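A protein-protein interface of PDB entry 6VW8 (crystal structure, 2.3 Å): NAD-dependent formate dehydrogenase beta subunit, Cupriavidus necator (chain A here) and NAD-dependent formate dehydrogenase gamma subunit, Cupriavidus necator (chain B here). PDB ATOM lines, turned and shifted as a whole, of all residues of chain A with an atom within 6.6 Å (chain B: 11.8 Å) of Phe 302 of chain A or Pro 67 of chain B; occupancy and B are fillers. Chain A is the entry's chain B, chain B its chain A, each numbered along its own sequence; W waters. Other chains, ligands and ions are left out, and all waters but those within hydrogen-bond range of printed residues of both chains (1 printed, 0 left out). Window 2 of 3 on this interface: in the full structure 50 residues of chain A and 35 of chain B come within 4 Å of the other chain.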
ATOM      1  N   TYR A 178     -12.906 -19.975 -12.631  1.00  0.00           N
ATOM      2  CA  TYR A 178     -13.416 -21.157 -11.964  1.00  0.00           C
ATOM      3  C   TYR A 178     -14.183 -22.050 -12.918  1.00  0.00           C
ATOM      4  O   TYR A 178     -14.879 -21.563 -13.819  1.00  0.00           O
ATOM      5  CB  TYR A 178     -14.337 -20.775 -10.812  1.00  0.00           C
ATOM      6  CG  TYR A 178     -13.631 -20.073  -9.689  1.00  0.00           C
ATOM      7  CD1 TYR A 178     -12.751 -20.773  -8.856  1.00  0.00           C
ATOM      8  CD2 TYR A 178     -13.849 -18.727  -9.440  1.00  0.00           C
ATOM      9  CE1 TYR A 178     -12.099 -20.144  -7.788  1.00  0.00           C
ATOM     10  CE2 TYR A 178     -13.200 -18.078  -8.382  1.00  0.00           C
ATOM     11  CZ  TYR A 178     -12.333 -18.795  -7.561  1.00  0.00           C
ATOM     12  OH  TYR A 178     -11.675 -18.172  -6.522  1.00  0.00           O
ATOM     13  N   TYR A 221     -14.941 -26.554  -8.469  1.00  0.00           N
ATOM     14  CA  TYR A 221     -15.798 -27.017  -7.388  1.00  0.00           C
ATOM     15  C   TYR A 221     -16.919 -27.873  -7.949  1.00  0.00           C
ATOM     16  O   TYR A 221     -17.538 -27.537  -8.961  1.00  0.00           O
ATOM     17  CB  TYR A 221     -16.392 -25.869  -6.591  1.00  0.00           C
ATOM     18  CG  TYR A 221     -15.348 -25.033  -5.907  1.00  0.00           C
ATOM     19  CD1 TYR A 221     -14.851 -25.396  -4.658  1.00  0.00           C
ATOM     20  CD2 TYR A 221     -14.848 -23.889  -6.505  1.00  0.00           C
ATOM     21  CE1 TYR A 221     -13.888 -24.636  -4.016  1.00  0.00           C
ATOM     22  CE2 TYR A 221     -13.875 -23.128  -5.870  1.00  0.00           C
ATOM     23  CZ  TYR A 221     -13.404 -23.514  -4.626  1.00  0.00           C
ATOM     24  OH  TYR A 221     -12.448 -22.767  -3.987  1.00  0.00           O
ATOM     25  N   GLU A 262     -12.264 -29.686  -5.662  1.00  0.00           N
ATOM     26  CA  GLU A 262     -12.793 -30.125  -4.384  1.00  0.00           C
ATOM     27  C   GLU A 262     -14.306 -30.217  -4.464  1.00  0.00           C
ATOM     28  O   GLU A 262     -14.956 -29.558  -5.299  1.00  0.00           O
ATOM     29  CB  GLU A 262     -12.362 -29.224  -3.230  1.00  0.00           C
ATOM     30  CG  GLU A 262     -12.952 -27.861  -3.197  1.00  0.00           C
ATOM     31  CD  GLU A 262     -12.373 -27.041  -2.039  1.00  0.00           C
ATOM     32  OE1 GLU A 262     -11.183 -26.665  -2.097  1.00  0.00           O
ATOM     33  OE2 GLU A 262     -13.088 -26.795  -1.049  1.00  0.00           O
ATOM     34  N   ARG A 264     -18.015 -29.827  -2.745  1.00  0.00           N
ATOM     35  CA  ARG A 264     -18.804 -29.103  -1.764  1.00  0.00           C
ATOM     36  C   ARG A 264     -20.163 -29.769  -1.645  1.00  0.00           C
ATOM     37  O   ARG A 264     -20.784 -30.106  -2.653  1.00  0.00           O
ATOM     38  CB  ARG A 264     -18.964 -27.626  -2.151  1.00  0.00           C
ATOM     39  CG  ARG A 264     -17.672 -26.794  -2.041  1.00  0.00           C
ATOM     40  CD  ARG A 264     -16.957 -26.927  -0.689  1.00  0.00           C
ATOM     41  NE  ARG A 264     -15.726 -26.119  -0.687  1.00  0.00           N
ATOM     42  CZ  ARG A 264     -15.673 -24.800  -0.508  1.00  0.00           C
ATOM     43  NH1 ARG A 264     -16.784 -24.079  -0.294  1.00  0.00           N
ATOM     44  NH2 ARG A 264     -14.495 -24.190  -0.571  1.00  0.00           N
ATOM     45  N   LEU A 279     -24.002 -20.449  -6.679  1.00  0.00           N
ATOM     46  CA  LEU A 279     -22.823 -19.642  -6.384  1.00  0.00           C
ATOM     47  C   LEU A 279     -22.936 -18.994  -5.007  1.00  0.00           C
ATOM     48  O   LEU A 279     -21.969 -18.981  -4.237  1.00  0.00           O
ATOM     49  CB  LEU A 279     -22.619 -18.571  -7.460  1.00  0.00           C
ATOM     50  CG  LEU A 279     -22.409 -19.005  -8.912  1.00  0.00           C
ATOM     51  CD1 LEU A 279     -22.015 -17.803  -9.784  1.00  0.00           C
ATOM     52  CD2 LEU A 279     -21.395 -20.132  -9.029  1.00  0.00           C
ATOM     53  N   LEU A 282     -22.073 -21.737  -2.464  1.00  0.00           N
ATOM     54  CA  LEU A 282     -20.632 -21.946  -2.424  1.00  0.00           C
ATOM     55  C   LEU A 282     -19.920 -20.885  -1.604  1.00  0.00           C
ATOM     56  O   LEU A 282     -18.943 -21.177  -0.911  1.00  0.00           O
ATOM     57  CB  LEU A 282     -20.076 -21.950  -3.837  1.00  0.00           C
ATOM     58  CG  LEU A 282     -20.316 -23.251  -4.582  1.00  0.00           C
ATOM     59  CD1 LEU A 282     -19.843 -23.073  -6.002  1.00  0.00           C
ATOM     60  CD2 LEU A 282     -19.564 -24.378  -3.869  1.00  0.00           C
ATOM     61  N   GLU A 283     -20.392 -19.652  -1.668  1.00  0.00           N
ATOM     62  CA  GLU A 283     -19.791 -18.540  -0.963  1.00  0.00           C
ATOM     63  C   GLU A 283     -20.219 -18.457   0.491  1.00  0.00           C
ATOM     64  O   GLU A 283     -19.889 -17.470   1.168  1.00  0.00           O
ATOM     65  CB  GLU A 283     -20.108 -17.240  -1.703  1.00  0.00           C
ATOM     66  CG  GLU A 283     -19.433 -17.230  -3.069  1.00  0.00           C
ATOM     67  CD  GLU A 283     -19.672 -15.971  -3.852  1.00  0.00           C
ATOM     68  OE1 GLU A 283     -19.862 -14.892  -3.225  1.00  0.00           O
ATOM     69  OE2 GLU A 283     -19.670 -16.081  -5.101  1.00  0.00           O
ATOM     70  N   GLY A 284     -20.964 -19.441   0.976  1.00  0.00           N
ATOM     71  CA  GLY A 284     -21.344 -19.461   2.371  1.00  0.00           C
ATOM     72  C   GLY A 284     -22.592 -18.680   2.702  1.00  0.00           C
ATOM     73  O   GLY A 284     -22.804 -18.347   3.866  1.00  0.00           O
ATOM     74  N   ARG A 285     -23.438 -18.391   1.727  1.00  0.00           N
ATOM     75  CA  ARG A 285     -24.622 -17.576   1.953  1.00  0.00           C
ATOM     76  C   ARG A 285     -25.873 -18.393   1.699  1.00  0.00           C
ATOM     77  O   ARG A 285     -25.823 -19.504   1.161  1.00  0.00           O
ATOM     78  CB  ARG A 285     -24.628 -16.340   1.050  1.00  0.00           C
ATOM     79  CG  ARG A 285     -23.926 -15.128   1.627  1.00  0.00           C
ATOM     80  CD  ARG A 285     -23.824 -14.002   0.559  1.00  0.00           C
ATOM     81  NE  ARG A 285     -22.421 -13.740   0.260  1.00  0.00           N
ATOM     82  CZ  ARG A 285     -21.869 -13.795  -0.944  1.00  0.00           C
ATOM     83  NH1 ARG A 285     -22.605 -14.069  -1.991  1.00  0.00           N
ATOM     84  NH2 ARG A 285     -20.571 -13.565  -1.089  1.00  0.00           N
ATOM     85  N   ARG A 290     -29.382 -14.691  -7.678  1.00  0.00           N
ATOM     86  CA  ARG A 290     -28.832 -13.351  -7.900  1.00  0.00           C
ATOM     87  C   ARG A 290     -29.548 -12.735  -9.090  1.00  0.00           C
ATOM     88  O   ARG A 290     -29.980 -13.438  -9.935  1.00  0.00           O
ATOM     89  CB  ARG A 290     -27.348 -13.347  -8.252  1.00  0.00           C
ATOM     90  CG  ARG A 290     -26.428 -14.103  -7.305  1.00  0.00           C
ATOM     91  CD  ARG A 290     -24.998 -14.115  -7.816  1.00  0.00           C
ATOM     92  NE  ARG A 290     -24.058 -14.430  -6.774  1.00  0.00           N
ATOM     93  CZ  ARG A 290     -22.758 -14.583  -6.916  1.00  0.00           C
ATOM     94  NH1 ARG A 290     -22.193 -14.455  -8.094  1.00  0.00           N
ATOM     95  NH2 ARG A 290     -22.021 -14.870  -5.871  1.00  0.00           N
ATOM     96  N   GLN A 299     -18.873 -12.665 -14.161  1.00  0.00           N
ATOM     97  CA  GLN A 299     -18.678 -12.354 -12.741  1.00  0.00           C
ATOM     98  C   GLN A 299     -19.484 -13.399 -11.986  1.00  0.00           C
ATOM     99  O   GLN A 299     -20.672 -13.214 -11.724  1.00  0.00           O
ATOM    100  CB  GLN A 299     -19.120 -10.923 -12.392  1.00  0.00           C
ATOM    101  CG  GLN A 299     -18.775  -9.861 -13.430  1.00  0.00           C
ATOM    102  CD  GLN A 299     -19.187  -8.453 -12.986  1.00  0.00           C
ATOM    103  OE1 GLN A 299     -18.919  -8.042 -11.856  1.00  0.00           O
ATOM    104  NE2 GLN A 299     -19.836  -7.713 -13.880  1.00  0.00           N
ATOM    105  N   GLY A 300     -18.851 -14.511 -11.665  1.00  0.00           N
ATOM    106  CA  GLY A 300     -19.584 -15.595 -11.049  1.00  0.00           C
ATOM    107  C   GLY A 300     -19.144 -15.821  -9.623  1.00  0.00           C
ATOM    108  O   GLY A 300     -19.446 -15.008  -8.736  1.00  0.00           O
ATOM    109  N   LEU A 301     -18.429 -16.926  -9.406  1.00  0.00           N
ATOM    110  CA  LEU A 301     -17.949 -17.265  -8.077  1.00  0.00           C
ATOM    111  C   LEU A 301     -16.948 -16.208  -7.621  1.00  0.00           C
ATOM    112  O   LEU A 301     -15.936 -15.963  -8.290  1.00  0.00           O
ATOM    113  CB  LEU A 301     -17.328 -18.667  -8.102  1.00  0.00           C
ATOM    114  CG  LEU A 301     -16.921 -19.303  -6.759  1.00  0.00           C
ATOM    115  CD1 LEU A 301     -18.130 -19.493  -5.804  1.00  0.00           C
ATOM    116  CD2 LEU A 301     -16.142 -20.646  -6.953  1.00  0.00           C
ATOM    117  N   PHE A 302     -17.249 -15.554  -6.497  1.00  0.00           N
ATOM    118  CA  PHE A 302     -16.441 -14.438  -5.990  1.00  0.00           C
ATOM    119  C   PHE A 302     -16.196 -13.386  -7.056  1.00  0.00           C
ATOM    120  O   PHE A 302     -15.131 -12.769  -7.108  1.00  0.00           O
ATOM    121  CB  PHE A 302     -15.103 -14.930  -5.420  1.00  0.00           C
ATOM    122  CG  PHE A 302     -15.269 -16.009  -4.410  1.00  0.00           C
ATOM    123  CD1 PHE A 302     -15.894 -15.739  -3.195  1.00  0.00           C
ATOM    124  CD2 PHE A 302     -14.858 -17.307  -4.684  1.00  0.00           C
ATOM    125  CE1 PHE A 302     -16.088 -16.755  -2.262  1.00  0.00           C
ATOM    126  CE2 PHE A 302     -15.053 -18.318  -3.764  1.00  0.00           C
ATOM    127  CZ  PHE A 302     -15.667 -18.035  -2.544  1.00  0.00           C
ATOM    128  N   GLY A 303     -17.203 -13.155  -7.897  1.00  0.00           N
ATOM    129  CA  GLY A 303     -17.062 -12.155  -8.940  1.00  0.00           C
ATOM    130  C   GLY A 303     -16.135 -12.544 -10.069  1.00  0.00           C
ATOM    131  O   GLY A 303     -15.869 -11.720 -10.941  1.00  0.00           O
ATOM    132  N   LYS A 304     -15.636 -13.795 -10.093  1.00  0.00           N
ATOM    133  CA  LYS A 304     -14.696 -14.197 -11.129  1.00  0.00           C
ATOM    134  C   LYS A 304     -15.423 -14.814 -12.312  1.00  0.00           C
ATOM    135  O   LYS A 304     -16.539 -15.340 -12.178  1.00  0.00           O
ATOM    136  CB  LYS A 304     -13.682 -15.212 -10.575  1.00  0.00           C
ATOM    137  CG  LYS A 304     -12.883 -14.725  -9.401  1.00  0.00           C
ATOM    138  CD  LYS A 304     -12.460 -13.279  -9.556  1.00  0.00           C
ATOM    139  CE  LYS A 304     -11.385 -12.937  -8.513  1.00  0.00           C
ATOM    140  NZ  LYS A 304     -10.270 -12.182  -9.141  1.00  0.00           N
ATOM    141  N   THR A 306     -16.576 -17.601 -14.540  1.00  0.00           N
ATOM    142  CA  THR A 306     -16.935 -18.912 -14.017  1.00  0.00           C
ATOM    143  C   THR A 306     -17.661 -19.691 -15.095  1.00  0.00           C
ATOM    144  O   THR A 306     -18.647 -19.193 -15.653  1.00  0.00           O
ATOM    145  CB  THR A 306     -17.882 -18.787 -12.817  1.00  0.00           C
ATOM    146  OG1 THR A 306     -17.363 -17.865 -11.856  1.00  0.00           O
ATOM    147  CG2 THR A 306     -18.189 -20.165 -12.189  1.00  0.00           C
ATOM    148  N   ILE B  59     -12.887 -27.304  14.655  1.00  0.00           N
ATOM    149  CA  ILE B  59     -13.476 -27.462  13.325  1.00  0.00           C
ATOM    150  C   ILE B  59     -13.447 -26.140  12.589  1.00  0.00           C
ATOM    151  O   ILE B  59     -13.018 -26.065  11.430  1.00  0.00           O
ATOM    152  CB  ILE B  59     -14.919 -27.988  13.417  1.00  0.00           C
ATOM    153  CG1 ILE B  59     -14.929 -29.493  13.714  1.00  0.00           C
ATOM    154  CG2 ILE B  59     -15.682 -27.663  12.122  1.00  0.00           C
ATOM    155  CD1 ILE B  59     -16.263 -30.006  14.199  1.00  0.00           C
ATOM    156  N   VAL B  60     -13.876 -25.073  13.278  1.00  0.00           N
ATOM    157  CA  VAL B  60     -14.018 -23.749  12.669  1.00  0.00           C
ATOM    158  C   VAL B  60     -12.656 -23.197  12.266  1.00  0.00           C
ATOM    159  O   VAL B  60     -12.475 -22.712  11.136  1.00  0.00           O
ATOM    160  CB  VAL B  60     -14.726 -22.796  13.660  1.00  0.00           C
ATOM    161  CG1 VAL B  60     -14.393 -21.356  13.370  1.00  0.00           C
ATOM    162  CG2 VAL B  60     -16.237 -23.008  13.673  1.00  0.00           C
ATOM    163  N   ALA B  61     -11.672 -23.283  13.189  1.00  0.00           N
ATOM    164  CA  ALA B  61     -10.346 -22.705  12.980  1.00  0.00           C
ATOM    165  C   ALA B  61      -9.593 -23.398  11.852  1.00  0.00           C
ATOM    166  O   ALA B  61      -8.768 -22.761  11.172  1.00  0.00           O
ATOM    167  CB  ALA B  61      -9.516 -22.779  14.273  1.00  0.00           C
ATOM    168  N   ALA B  62      -9.827 -24.703  11.665  1.00  0.00           N
ATOM    169  CA  ALA B  62      -9.207 -25.415  10.549  1.00  0.00           C
ATOM    170  C   ALA B  62      -9.763 -24.943   9.212  1.00  0.00           C
ATOM    171  O   ALA B  62      -9.089 -25.064   8.178  1.00  0.00           O
ATOM    172  CB  ALA B  62      -9.413 -26.926  10.704  1.00  0.00           C
ATOM    173  N   ARG B  63     -10.968 -24.391   9.210  1.00  0.00           N
ATOM    174  CA  ARG B  63     -11.658 -24.070   7.973  1.00  0.00           C
ATOM    175  C   ARG B  63     -11.736 -22.573   7.724  1.00  0.00           C
ATOM    176  O   ARG B  63     -12.341 -22.142   6.727  1.00  0.00           O
ATOM    177  CB  ARG B  63     -13.058 -24.691   7.996  1.00  0.00           C
ATOM    178  CG  ARG B  63     -13.067 -26.175   7.662  1.00  0.00           C
ATOM    179  CD  ARG B  63     -14.306 -26.891   8.194  1.00  0.00           C
ATOM    180  NE  ARG B  63     -14.125 -28.324   8.028  1.00  0.00           N
ATOM    181  CZ  ARG B  63     -13.462 -29.090   8.888  1.00  0.00           C
ATOM    182  NH1 ARG B  63     -12.950 -28.551   9.991  1.00  0.00           N
ATOM    183  NH2 ARG B  63     -13.320 -30.391   8.654  1.00  0.00           N
ATOM    184  N   GLN B  64     -11.139 -21.763   8.600  1.00  0.00           N
ATOM    185  CA  GLN B  64     -11.467 -20.342   8.607  1.00  0.00           C
ATOM    186  C   GLN B  64     -10.919 -19.592   7.391  1.00  0.00           C
ATOM    187  O   GLN B  64     -11.430 -18.512   7.066  1.00  0.00           O
ATOM    188  CB  GLN B  64     -10.971 -19.712   9.908  1.00  0.00           C
ATOM    189  CG  GLN B  64      -9.466 -19.537   9.998  1.00  0.00           C
ATOM    190  CD  GLN B  64      -9.094 -18.535  11.066  1.00  0.00           C
ATOM    191  OE1 GLN B  64      -9.601 -18.605  12.185  1.00  0.00           O
ATOM    192  NE2 GLN B  64      -8.242 -17.565  10.715  1.00  0.00           N
ATOM    193  N   ASP B  65      -9.948 -20.154   6.670  1.00  0.00           N
ATOM    194  CA  ASP B  65      -9.445 -19.499   5.468  1.00  0.00           C
ATOM    195  C   ASP B  65      -9.974 -20.123   4.182  1.00  0.00           C
ATOM    196  O   ASP B  65      -9.575 -19.688   3.090  1.00  0.00           O
ATOM    197  CB  ASP B  65      -7.916 -19.525   5.452  1.00  0.00           C
ATOM    198  CG  ASP B  65      -7.311 -18.450   6.338  1.00  0.00           C
ATOM    199  OD1 ASP B  65      -8.086 -17.629   6.867  1.00  0.00           O
ATOM    200  OD2 ASP B  65      -6.072 -18.424   6.523  1.00  0.00           O
ATOM    201  N   ILE B  66     -10.865 -21.105   4.278  1.00  0.00           N
ATOM    202  CA  ILE B  66     -11.440 -21.705   3.076  1.00  0.00           C
ATOM    203  C   ILE B  66     -12.418 -20.721   2.430  1.00  0.00           C
ATOM    204  O   ILE B  66     -13.228 -20.089   3.140  1.00  0.00           O
ATOM    205  CB  ILE B  66     -12.127 -23.022   3.418  1.00  0.00           C
ATOM    206  CG1 ILE B  66     -11.066 -24.081   3.724  1.00  0.00           C
ATOM    207  CG2 ILE B  66     -13.036 -23.486   2.264  1.00  0.00           C
ATOM    208  CD1 ILE B  66     -11.635 -25.364   4.177  1.00  0.00           C
ATOM    209  N   PRO B  67     -12.363 -20.537   1.112  1.00  0.00           N
ATOM    210  CA  PRO B  67     -13.360 -19.694   0.425  1.00  0.00           C
ATOM    211  C   PRO B  67     -14.762 -20.277   0.541  1.00  0.00           C
ATOM    212  O   PRO B  67     -15.001 -21.435   0.194  1.00  0.00           O
ATOM    213  CB  PRO B  67     -12.877 -19.684  -1.031  1.00  0.00           C
ATOM    214  CG  PRO B  67     -11.414 -20.082  -0.973  1.00  0.00           C
ATOM    215  CD  PRO B  67     -11.289 -21.000   0.213  1.00  0.00           C
ATOM    216  N   GLY B  68     -15.695 -19.467   1.033  1.00  0.00           N
ATOM    217  CA  GLY B  68     -17.048 -19.944   1.279  1.00  0.00           C
ATOM    218  C   GLY B  68     -17.099 -21.026   2.342  1.00  0.00           C
ATOM    219  O   GLY B  68     -17.784 -22.046   2.200  1.00  0.00           O
ATOM    220  N   ALA B  69     -16.397 -20.767   3.447  1.00  0.00           N
ATOM    221  CA  ALA B  69     -16.181 -21.767   4.482  1.00  0.00           C
ATOM    222  C   ALA B  69     -17.443 -22.138   5.252  1.00  0.00           C
ATOM    223  O   ALA B  69     -17.452 -23.191   5.897  1.00  0.00           O
ATOM    224  CB  ALA B  69     -15.118 -21.256   5.470  1.00  0.00           C
ATOM    225  N   LEU B  70     -18.483 -21.296   5.239  1.00  0.00           N
ATOM    226  CA  LEU B  70     -19.577 -21.451   6.205  1.00  0.00           C
ATOM    227  C   LEU B  70     -20.215 -22.840   6.138  1.00  0.00           C
ATOM    228  O   LEU B  70     -20.372 -23.509   7.170  1.00  0.00           O
ATOM    229  CB  LEU B  70     -20.640 -20.365   6.003  1.00  0.00           C
ATOM    230  CG  LEU B  70     -21.777 -20.415   7.035  1.00  0.00           C
ATOM    231  CD1 LEU B  70     -21.201 -20.735   8.420  1.00  0.00           C
ATOM    232  CD2 LEU B  70     -22.576 -19.114   7.073  1.00  0.00           C
ATOM    233  N   LEU B  71     -20.630 -23.278   4.936  1.00  0.00           N
ATOM    234  CA  LEU B  71     -21.323 -24.563   4.829  1.00  0.00           C
ATOM    235  C   LEU B  71     -20.413 -25.722   5.188  1.00  0.00           C
ATOM    236  O   LEU B  71     -20.852 -26.609   5.941  1.00  0.00           O
ATOM    237  CB  LEU B  71     -21.925 -24.745   3.428  1.00  0.00           C
ATOM    238  CG  LEU B  71     -23.421 -24.467   3.288  1.00  0.00           C
ATOM    239  CD1 LEU B  71     -23.696 -22.947   3.307  1.00  0.00           C
ATOM    240  CD2 LEU B  71     -23.943 -25.102   1.992  1.00  0.00           C
ATOM    241  N   PRO B  72     -19.176 -25.818   4.670  1.00  0.00           N
ATOM    242  CA  PRO B  72     -18.268 -26.866   5.173  1.00  0.00           C
ATOM    243  C   PRO B  72     -18.139 -26.861   6.677  1.00  0.00           C
ATOM    244  O   PRO B  72     -18.163 -27.924   7.304  1.00  0.00           O
ATOM    245  CB  PRO B  72     -16.951 -26.533   4.472  1.00  0.00           C
ATOM    246  CG  PRO B  72     -17.425 -26.009   3.098  1.00  0.00           C
ATOM    247  CD  PRO B  72     -18.615 -25.140   3.482  1.00  0.00           C
ATOM    248  N   ILE B  73     -18.039 -25.690   7.292  1.00  0.00           N
ATOM    249  CA  ILE B  73     -17.998 -25.639   8.750  1.00  0.00           C
ATOM    250  C   ILE B  73     -19.296 -26.200   9.326  1.00  0.00           C
ATOM    251  O   ILE B  73     -19.292 -27.033  10.241  1.00  0.00           O
ATOM    252  CB  ILE B  73     -17.735 -24.193   9.212  1.00  0.00           C
ATOM    253  CG1 ILE B  73     -16.265 -23.830   8.945  1.00  0.00           C
ATOM    254  CG2 ILE B  73     -18.168 -24.001  10.669  1.00  0.00           C
ATOM    255  CD1 ILE B  73     -15.842 -22.443   9.360  1.00  0.00           C
ATOM    256  N   LEU B  74     -20.426 -25.795   8.760  1.00  0.00           N
ATOM    257  CA  LEU B  74     -21.701 -26.267   9.281  1.00  0.00           C
ATOM    258  C   LEU B  74     -21.831 -27.768   9.096  1.00  0.00           C
ATOM    259  O   LEU B  74     -22.332 -28.468   9.982  1.00  0.00           O
ATOM    260  CB  LEU B  74     -22.852 -25.520   8.607  1.00  0.00           C
ATOM    261  CG  LEU B  74     -22.951 -24.020   8.934  1.00  0.00           C
ATOM    262  CD1 LEU B  74     -24.064 -23.313   8.117  1.00  0.00           C
ATOM    263  CD2 LEU B  74     -23.189 -23.790  10.414  1.00  0.00           C
ATOM    264  N   HIS B  75     -21.353 -28.285   7.963  1.00  0.00           N
ATOM    265  CA  HIS B  75     -21.398 -29.726   7.735  1.00  0.00           C
ATOM    266  C   HIS B  75     -20.537 -30.460   8.746  1.00  0.00           C
ATOM    267  O   HIS B  75     -20.959 -31.480   9.308  1.00  0.00           O
ATOM    268  CB  HIS B  75     -20.964 -30.064   6.304  1.00  0.00           C
ATOM    269  CG  HIS B  75     -22.068 -29.930   5.305  1.00  0.00           C
ATOM    270  ND1 HIS B  75     -23.327 -30.451   5.518  1.00  0.00           N
ATOM    271  CD2 HIS B  75     -22.119 -29.307   4.101  1.00  0.00           C
ATOM    272  CE1 HIS B  75     -24.096 -30.180   4.476  1.00  0.00           C
ATOM    273  NE2 HIS B  75     -23.385 -29.488   3.603  1.00  0.00           N
ATOM    274  N   ALA B  95     -14.772 -16.062  13.589  1.00  0.00           N
ATOM    275  CA  ALA B  95     -13.683 -16.541  12.760  1.00  0.00           C
ATOM    276  C   ALA B  95     -13.902 -16.213  11.285  1.00  0.00           C
ATOM    277  O   ALA B  95     -12.941 -16.181  10.513  1.00  0.00           O
ATOM    278  CB  ALA B  95     -13.534 -18.057  12.942  1.00  0.00           C
ATOM    279  N   LEU B  96     -15.140 -15.953  10.872  1.00  0.00           N
ATOM    280  CA  LEU B  96     -15.453 -15.673   9.473  1.00  0.00           C
ATOM    281  C   LEU B  96     -15.668 -14.188   9.189  1.00  0.00           C
ATOM    282  O   LEU B  96     -15.912 -13.818   8.031  1.00  0.00           O
ATOM    283  CB  LEU B  96     -16.697 -16.466   9.052  1.00  0.00           C
ATOM    284  CG  LEU B  96     -16.514 -17.836   8.392  1.00  0.00           C
ATOM    285  CD1 LEU B  96     -15.447 -18.653   9.064  1.00  0.00           C
ATOM    286  CD2 LEU B  96     -17.837 -18.625   8.272  1.00  0.00           C
ATOM    287  N   LEU B  98     -18.167 -12.440  10.040  1.00  0.00           N
ATOM    288  CA  LEU B  98     -19.568 -12.398   9.682  1.00  0.00           C
ATOM    289  C   LEU B  98     -20.355 -12.030  10.929  1.00  0.00           C
ATOM    290  O   LEU B  98     -19.870 -12.158  12.055  1.00  0.00           O
ATOM    291  CB  LEU B  98     -20.048 -13.761   9.142  1.00  0.00           C
ATOM    292  CG  LEU B  98     -19.585 -14.289   7.768  1.00  0.00           C
ATOM    293  CD1 LEU B  98     -20.262 -15.619   7.438  1.00  0.00           C
ATOM    294  CD2 LEU B  98     -19.826 -13.288   6.630  1.00  0.00           C
HETATM  295  O   HOH W   1     -20.127 -22.340   1.350  1.00  0.00           O
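The guanidinium group (NH2) of Arg 264 of chain A is in hydrogen-bond range of the backbone carbonyl oxygen (O) of Pro 67 of chain B (2.9 Å). O of Leu 282 of chain A sits close to O of Gly 68 of chain B, at 3.4 Å. O of Gly 68 of chain B is in hydrogen-bond range of NH1 of Arg 264 of chain A (3.4 Å).
Of the 17 printed residues of chain A, 5 touch a printed residue of chain B. Hydrophobic or aromatic side chains of chain A within 4 Å of the printed part of chain B: Phe 302. Printed residues of chain B that touch a printed residue of chain A: Ile 66, Pro 67, Gly 68, Leu 70 and Pro 72.
Water W1 lies within hydrogen-bond range of the backbone carbonyl oxygen of Gly 68 of chain B (2.5 Å), the backbone carbonyl oxygen of Leu 282 of chain A (2.8 Å) and the backbone NH of Gly 284 of chain A (3.0 Å).
Of chain A, only Arg 264 and Phe 302 come within 4 Å of Pro 67 of chain B. Leu 301 of chain A touches none of the printed residues of chain B. Gly 303 of chain A touches none of the printed residues of chain B. No residue of chain B comes within 4 Å of Lys 304 of chain A. Printed residues of chain B within 4 Å of Arg 264 of chain A: Ile 66, Pro 67, Gly 68 and Pro 72. Printed residues of chain B within 4 Å of Gly 284 of chain A: Gly 68 (3.96 Å) and Leu 70 (3.3 Å). Of the printed residues of chain A, Leu 70 of chain B touches Gly 284. Ile 59 of chain B touches none of the printed residues of chain A. Gln 64 of chain B touches none of the printed residues of chain A. The nearest printed residue of chain B that does not touch Gly 284 of chain A is Leu 71 of chain B (4.3 Å).
Among the printed residues, pairs that only touch across the chains: Arg 264 of chain A with Ile 66 of chain B, Gly 284 of chain A with Leu 70 of chain B, Phe 302 of chain A with Pro 67 of chain B, Glu 283 of chain A with Gly 68 of chain B, Phe 302 of chain A with Gly 68 of chain B, Arg 264 of chain A with Pro 72 of chain B and Gly 284 of chain A with Gly 68 of chain B.
OE2 of Glu 262 of chain A is in salt-bridge range of NE of Arg 264 of chain A, at 2.7 Å. The side-chain carboxylate (OE2) of Glu 283 of chain A lies within hydrogen-bond range of the backbone NH (N) of Phe 302 of chain A (2.8 Å). OE1 of Glu 283 of chain A is in salt-bridge range of NH2 of Arg 285 of chain A (2.6 Å). NH2 of Arg 290 of chain A lies within salt-bridge range of OE2 of Glu 283 of chain A (2.8 Å).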
